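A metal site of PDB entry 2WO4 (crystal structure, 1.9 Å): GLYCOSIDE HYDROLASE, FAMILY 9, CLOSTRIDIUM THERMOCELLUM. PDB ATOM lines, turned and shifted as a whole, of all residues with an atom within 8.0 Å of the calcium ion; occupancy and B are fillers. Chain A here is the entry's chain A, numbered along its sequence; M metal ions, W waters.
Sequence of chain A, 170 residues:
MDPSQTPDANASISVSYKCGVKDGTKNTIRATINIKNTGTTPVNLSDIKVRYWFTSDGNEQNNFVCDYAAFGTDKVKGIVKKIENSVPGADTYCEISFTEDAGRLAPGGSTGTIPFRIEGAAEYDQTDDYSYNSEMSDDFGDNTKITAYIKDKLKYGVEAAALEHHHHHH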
ATOM      1  N   ILE A  29      14.126  27.687  35.629  1.00  0.00           N
ATOM      2  CA  ILE A  29      13.800  27.865  34.221  1.00  0.00           C
ATOM      3  C   ILE A  29      12.302  28.158  34.162  1.00  0.00           C
ATOM      4  O   ILE A  29      11.541  27.326  34.661  1.00  0.00           O
ATOM      5  CB  ILE A  29      14.131  26.601  33.406  1.00  0.00           C
ATOM      6  CG1 ILE A  29      15.628  26.403  33.342  1.00  0.00           C
ATOM      7  CG2 ILE A  29      13.609  26.714  31.991  1.00  0.00           C
ATOM      8  CD1 ILE A  29      16.045  24.993  32.801  1.00  0.00           C
ATOM      9  N   TRP A  53      14.197  20.534  25.967  1.00  0.00           N
ATOM     10  CA  TRP A  53      15.569  20.018  26.001  1.00  0.00           C
ATOM     11  C   TRP A  53      16.568  21.033  26.501  1.00  0.00           C
ATOM     12  O   TRP A  53      16.553  22.204  26.023  1.00  0.00           O
ATOM     13  CB  TRP A  53      15.960  19.653  24.592  1.00  0.00           C
ATOM     14  CG  TRP A  53      14.986  18.749  23.776  1.00  0.00           C
ATOM     15  CD1 TRP A  53      13.883  19.126  23.125  1.00  0.00           C
ATOM     16  CD2 TRP A  53      15.112  17.323  23.561  1.00  0.00           C
ATOM     17  NE1 TRP A  53      13.284  18.044  22.525  1.00  0.00           N
ATOM     18  CE2 TRP A  53      14.023  16.929  22.782  1.00  0.00           C
ATOM     19  CE3 TRP A  53      16.049  16.367  23.984  1.00  0.00           C
ATOM     20  CZ2 TRP A  53      13.816  15.588  22.371  1.00  0.00           C
ATOM     21  CZ3 TRP A  53      15.851  15.032  23.603  1.00  0.00           C
ATOM     22  CH2 TRP A  53      14.744  14.667  22.797  1.00  0.00           C
ATOM     23  N   PHE A  54      17.427  20.650  27.455  1.00  0.00           N
ATOM     24  CA  PHE A  54      18.346  21.616  28.079  1.00  0.00           C
ATOM     25  C   PHE A  54      19.593  20.961  28.657  1.00  0.00           C
ATOM     26  O   PHE A  54      19.683  19.745  28.733  1.00  0.00           O
ATOM     27  CB  PHE A  54      17.632  22.421  29.206  1.00  0.00           C
ATOM     28  CG  PHE A  54      17.155  21.592  30.395  1.00  0.00           C
ATOM     29  CD1 PHE A  54      17.725  21.731  31.603  1.00  0.00           C
ATOM     30  CD2 PHE A  54      16.053  20.755  30.300  1.00  0.00           C
ATOM     31  CE1 PHE A  54      17.245  21.040  32.752  1.00  0.00           C
ATOM     32  CE2 PHE A  54      15.603  20.010  31.422  1.00  0.00           C
ATOM     33  CZ  PHE A  54      16.208  20.212  32.672  1.00  0.00           C
ATOM     34  N   THR A  55      20.552  21.808  28.998  1.00  0.00           N
ATOM     35  CA  THR A  55      21.688  21.362  29.742  1.00  0.00           C
ATOM     36  C   THR A  55      21.527  21.762  31.204  1.00  0.00           C
ATOM     37  O   THR A  55      21.360  22.956  31.556  1.00  0.00           O
ATOM     38  CB  THR A  55      23.015  21.910  29.203  1.00  0.00           C
ATOM     39  OG1 THR A  55      22.959  23.337  28.989  1.00  0.00           O
ATOM     40  CG2 THR A  55      23.407  21.302  27.826  1.00  0.00           C
ATOM     41  N   SER A  56      21.650  20.764  32.067  1.00  0.00           N
ATOM     42  CA  SER A  56      21.344  20.997  33.489  1.00  0.00           C
ATOM     43  C   SER A  56      22.480  21.646  34.303  1.00  0.00           C
ATOM     44  O   SER A  56      22.301  22.060  35.475  1.00  0.00           O
ATOM     45  CB  SER A  56      20.838  19.705  34.124  1.00  0.00           C
ATOM     46  OG  SER A  56      21.821  18.719  34.138  1.00  0.00           O
ATOM     47  N   ASP A  57      23.627  21.803  33.660  1.00  0.00           N
ATOM     48  CA  ASP A  57      24.746  22.587  34.183  1.00  0.00           C
ATOM     49  C   ASP A  57      25.211  22.092  35.546  1.00  0.00           C
ATOM     50  O   ASP A  57      25.458  22.874  36.426  1.00  0.00           O
ATOM     51  CB  ASP A  57      24.390  24.086  34.242  1.00  0.00           C
ATOM     52  CG  ASP A  57      23.806  24.620  32.943  1.00  0.00           C
ATOM     53  OD1 ASP A  57      24.240  24.166  31.896  1.00  0.00           O
ATOM     54  OD2 ASP A  57      22.869  25.444  32.944  1.00  0.00           O
ATOM     55  N   GLY A  58      25.250  20.789  35.720  1.00  0.00           N
ATOM     56  CA  GLY A  58      25.704  20.237  36.989  1.00  0.00           C
ATOM     57  C   GLY A  58      24.606  19.862  37.994  1.00  0.00           C
ATOM     58  O   GLY A  58      24.860  19.071  38.931  1.00  0.00           O
ATOM     59  N   ASN A  59      23.390  20.371  37.774  1.00  0.00           N
ATOM     60  CA  ASN A  59      22.273  20.054  38.674  1.00  0.00           C
ATOM     61  C   ASN A  59      21.908  18.615  38.521  1.00  0.00           C
ATOM     62  O   ASN A  59      21.513  18.183  37.447  1.00  0.00           O
ATOM     63  CB  ASN A  59      21.053  20.957  38.312  1.00  0.00           C
ATOM     64  CG  ASN A  59      21.143  22.311  38.946  1.00  0.00           C
ATOM     65  OD1 ASN A  59      21.238  22.422  40.153  1.00  0.00           O
ATOM     66  ND2 ASN A  59      21.178  23.354  38.133  1.00  0.00           N
ATOM     67  N   GLY A  89      23.362  21.108  23.076  1.00  0.00           N
ATOM     68  CA  GLY A  89      22.339  21.839  23.792  1.00  0.00           C
ATOM     69  C   GLY A  89      21.479  21.032  24.734  1.00  0.00           C
ATOM     70  O   GLY A  89      20.535  21.555  25.327  1.00  0.00           O
ATOM     71  N   ALA A  90      21.752  19.719  24.897  1.00  0.00           N
ATOM     72  CA  ALA A  90      20.909  18.951  25.821  1.00  0.00           C
ATOM     73  C   ALA A  90      21.644  17.774  26.416  1.00  0.00           C
ATOM     74  O   ALA A  90      22.123  16.915  25.668  1.00  0.00           O
ATOM     75  CB  ALA A  90      19.638  18.438  25.089  1.00  0.00           C
ATOM     76  N   ASP A  91      21.698  17.747  27.728  1.00  0.00           N
ATOM     77  CA  ASP A  91      21.996  16.549  28.440  1.00  0.00           C
ATOM     78  C   ASP A  91      20.823  16.026  29.300  1.00  0.00           C
ATOM     79  O   ASP A  91      20.941  15.006  30.001  1.00  0.00           O
ATOM     80  CB  ASP A  91      23.231  16.704  29.280  1.00  0.00           C
ATOM     81  CG  ASP A  91      23.146  17.760  30.360  1.00  0.00           C
ATOM     82  OD1 ASP A  91      22.037  18.243  30.733  1.00  0.00           O
ATOM     83  OD2 ASP A  91      24.231  18.063  30.942  1.00  0.00           O
ATOM     84  N   GLU A 123      22.615  27.262  39.951  1.00  0.00           N
ATOM     85  CA  GLU A 123      22.330  28.107  38.849  1.00  0.00           C
ATOM     86  C   GLU A 123      22.281  27.372  37.472  1.00  0.00           C
ATOM     87  O   GLU A 123      23.047  26.460  37.228  1.00  0.00           O
ATOM     88  CB  GLU A 123      23.389  29.186  38.916  1.00  0.00           C
ATOM     89  CG  GLU A 123      23.488  30.169  37.811  1.00  0.00           C
ATOM     90  CD  GLU A 123      24.497  31.309  38.168  1.00  0.00           C
ATOM     91  OE1 GLU A 123      24.734  31.574  39.384  1.00  0.00           O
ATOM     92  OE2 GLU A 123      25.026  31.943  37.232  1.00  0.00           O
ATOM     93  N   TYR A 124      21.331  27.771  36.627  1.00  0.00           N
ATOM     94  CA  TYR A 124      21.227  27.383  35.230  1.00  0.00           C
ATOM     95  C   TYR A 124      21.758  28.475  34.347  1.00  0.00           C
ATOM     96  O   TYR A 124      21.465  29.661  34.539  1.00  0.00           O
ATOM     97  CB  TYR A 124      19.757  27.175  34.860  1.00  0.00           C
ATOM     98  CG  TYR A 124      19.121  25.946  35.420  1.00  0.00           C
ATOM     99  CD1 TYR A 124      17.984  26.052  36.251  1.00  0.00           C
ATOM    100  CD2 TYR A 124      19.598  24.688  35.167  1.00  0.00           C
ATOM    101  CE1 TYR A 124      17.323  24.941  36.752  1.00  0.00           C
ATOM    102  CE2 TYR A 124      18.919  23.512  35.674  1.00  0.00           C
ATOM    103  CZ  TYR A 124      17.754  23.682  36.472  1.00  0.00           C
ATOM    104  OH  TYR A 124      17.077  22.639  36.999  1.00  0.00           O
ATOM    105  N   ASP A 125      22.515  28.132  33.330  1.00  0.00           N
ATOM    106  CA  ASP A 125      22.755  29.083  32.271  1.00  0.00           C
ATOM    107  C   ASP A 125      21.878  28.588  31.164  1.00  0.00           C
ATOM    108  O   ASP A 125      22.064  27.484  30.676  1.00  0.00           O
ATOM    109  CB  ASP A 125      24.229  29.052  31.868  1.00  0.00           C
ATOM    110  CG  ASP A 125      24.541  29.936  30.698  1.00  0.00           C
ATOM    111  OD1 ASP A 125      23.721  30.648  30.086  1.00  0.00           O
ATOM    112  OD2 ASP A 125      25.727  29.923  30.352  1.00  0.00           O
ATOM    113  N   GLN A 126      20.900  29.405  30.765  1.00  0.00           N
ATOM    114  CA  GLN A 126      19.934  28.979  29.742  1.00  0.00           C
ATOM    115  C   GLN A 126      20.395  29.186  28.318  1.00  0.00           C
ATOM    116  O   GLN A 126      19.834  28.582  27.447  1.00  0.00           O
ATOM    117  CB  GLN A 126      18.585  29.706  30.023  1.00  0.00           C
ATOM    118  CG  GLN A 126      18.079  29.337  31.399  1.00  0.00           C
ATOM    119  CD  GLN A 126      16.646  29.789  31.617  1.00  0.00           C
ATOM    120  OE1 GLN A 126      15.786  29.429  30.800  1.00  0.00           O
ATOM    121  NE2 GLN A 126      16.410  30.645  32.635  1.00  0.00           N
ATOM    122  N   THR A 127      21.486  29.963  28.077  1.00  0.00           N
ATOM    123  CA  THR A 127      21.948  30.209  26.706  1.00  0.00           C
ATOM    124  C   THR A 127      22.435  28.965  25.990  1.00  0.00           C
ATOM    125  O   THR A 127      22.331  28.863  24.764  1.00  0.00           O
ATOM    126  CB  THR A 127      23.068  31.326  26.589  1.00  0.00           C
ATOM    127  OG1 THR A 127      24.073  31.109  27.603  1.00  0.00           O
ATOM    128  CG2 THR A 127      22.404  32.700  26.706  1.00  0.00           C
ATOM    129  N   ASP A 128      22.890  27.990  26.756  1.00  0.00           N
ATOM    130  CA  ASP A 128      23.328  26.698  26.181  1.00  0.00           C
ATOM    131  C   ASP A 128      22.284  25.580  26.271  1.00  0.00           C
ATOM    132  O   ASP A 128      22.612  24.404  26.329  1.00  0.00           O
ATOM    133  CB  ASP A 128      24.653  26.269  26.819  1.00  0.00           C
ATOM    134  CG  ASP A 128      24.596  26.060  28.309  1.00  0.00           C
ATOM    135  OD1 ASP A 128      23.530  26.060  28.985  1.00  0.00           O
ATOM    136  OD2 ASP A 128      25.671  25.831  28.873  1.00  0.00           O
ATOM    137  N   ASP A 129      21.005  25.957  26.249  1.00  0.00           N
ATOM    138  CA  ASP A 129      19.940  25.006  26.273  1.00  0.00           C
ATOM    139  C   ASP A 129      19.310  25.016  24.940  1.00  0.00           C
ATOM    140  O   ASP A 129      18.883  26.062  24.469  1.00  0.00           O
ATOM    141  CB  ASP A 129      18.883  25.379  27.278  1.00  0.00           C
ATOM    142  CG  ASP A 129      19.358  25.321  28.682  1.00  0.00           C
ATOM    143  OD1 ASP A 129      20.447  24.767  29.050  1.00  0.00           O
ATOM    144  OD2 ASP A 129      18.600  25.839  29.540  1.00  0.00           O
ATOM    145  N   TYR A 130      19.142  23.827  24.325  1.00  0.00           N
ATOM    146  CA  TYR A 130      18.605  23.698  23.004  1.00  0.00           C
ATOM    147  C   TYR A 130      17.254  24.383  22.819  1.00  0.00           C
ATOM    148  O   TYR A 130      17.005  25.061  21.783  1.00  0.00           O
ATOM    149  CB  TYR A 130      18.402  22.192  22.711  1.00  0.00           C
ATOM    150  CG  TYR A 130      17.886  21.814  21.410  1.00  0.00           C
ATOM    151  CD1 TYR A 130      18.686  21.850  20.287  1.00  0.00           C
ATOM    152  CD2 TYR A 130      16.526  21.440  21.230  1.00  0.00           C
ATOM    153  CE1 TYR A 130      18.196  21.503  19.056  1.00  0.00           C
ATOM    154  CE2 TYR A 130      16.048  21.042  20.025  1.00  0.00           C
ATOM    155  CZ  TYR A 130      16.883  21.087  18.899  1.00  0.00           C
ATOM    156  OH  TYR A 130      16.426  20.737  17.636  1.00  0.00           O
ATOM    157  N   TYR A 132      15.774  26.752  24.579  1.00  0.00           N
ATOM    158  CA  TYR A 132      15.666  28.176  25.013  1.00  0.00           C
ATOM    159  C   TYR A 132      15.666  29.113  23.803  1.00  0.00           C
ATOM    160  O   TYR A 132      16.499  28.999  22.897  1.00  0.00           O
ATOM    161  CB  TYR A 132      16.768  28.506  25.988  1.00  0.00           C
ATOM    162  CG  TYR A 132      16.878  29.949  26.495  1.00  0.00           C
ATOM    163  CD1 TYR A 132      15.989  30.466  27.476  1.00  0.00           C
ATOM    164  CD2 TYR A 132      17.882  30.791  26.006  1.00  0.00           C
ATOM    165  CE1 TYR A 132      16.119  31.769  27.961  1.00  0.00           C
ATOM    166  CE2 TYR A 132      18.010  32.095  26.472  1.00  0.00           C
ATOM    167  CZ  TYR A 132      17.164  32.573  27.435  1.00  0.00           C
ATOM    168  OH  TYR A 132      17.353  33.835  27.842  1.00  0.00           O
HETATM  169 CA    CA M   1      22.185  25.064  30.641  1.00  0.00          CA
HETATM  170  O   HOH W   1      20.002  25.555  31.863  1.00  0.00           O
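The side-chain carboxylate (OD1) of Asp 125 is in hydrogen-bond range of the side-chain hydroxyl (OG1) of Thr 127, 2.5 Å away.
Five residues have an atom within 4 Å of the calcium ion: Thr 55, Asp 57, Asp 125, Asp 128 and Asp 129.
The nearest printed residue that does not touch the calcium ion is Gln 126 (4.5 Å).
The calcium ion is bound by the side-chain carboxylate (OD1) of Asp 128 (2.4 Å), the side-chain carboxylate (OD1) of Asp 129 (2.4 Å), the backbone carbonyl oxygen (O) of Asp 125 (2.4 Å), the side-chain carboxylate (OD2) of Asp 57 (2.4 Å), the backbone carbonyl oxygen (O) of Thr 55 (2.4 Å), the side-chain hydroxyl (OG1) of Thr 55 (2.5 Å), water W1 (2.5 Å) and the side-chain carboxylate (OD1) of Asp 57 (2.6 Å).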
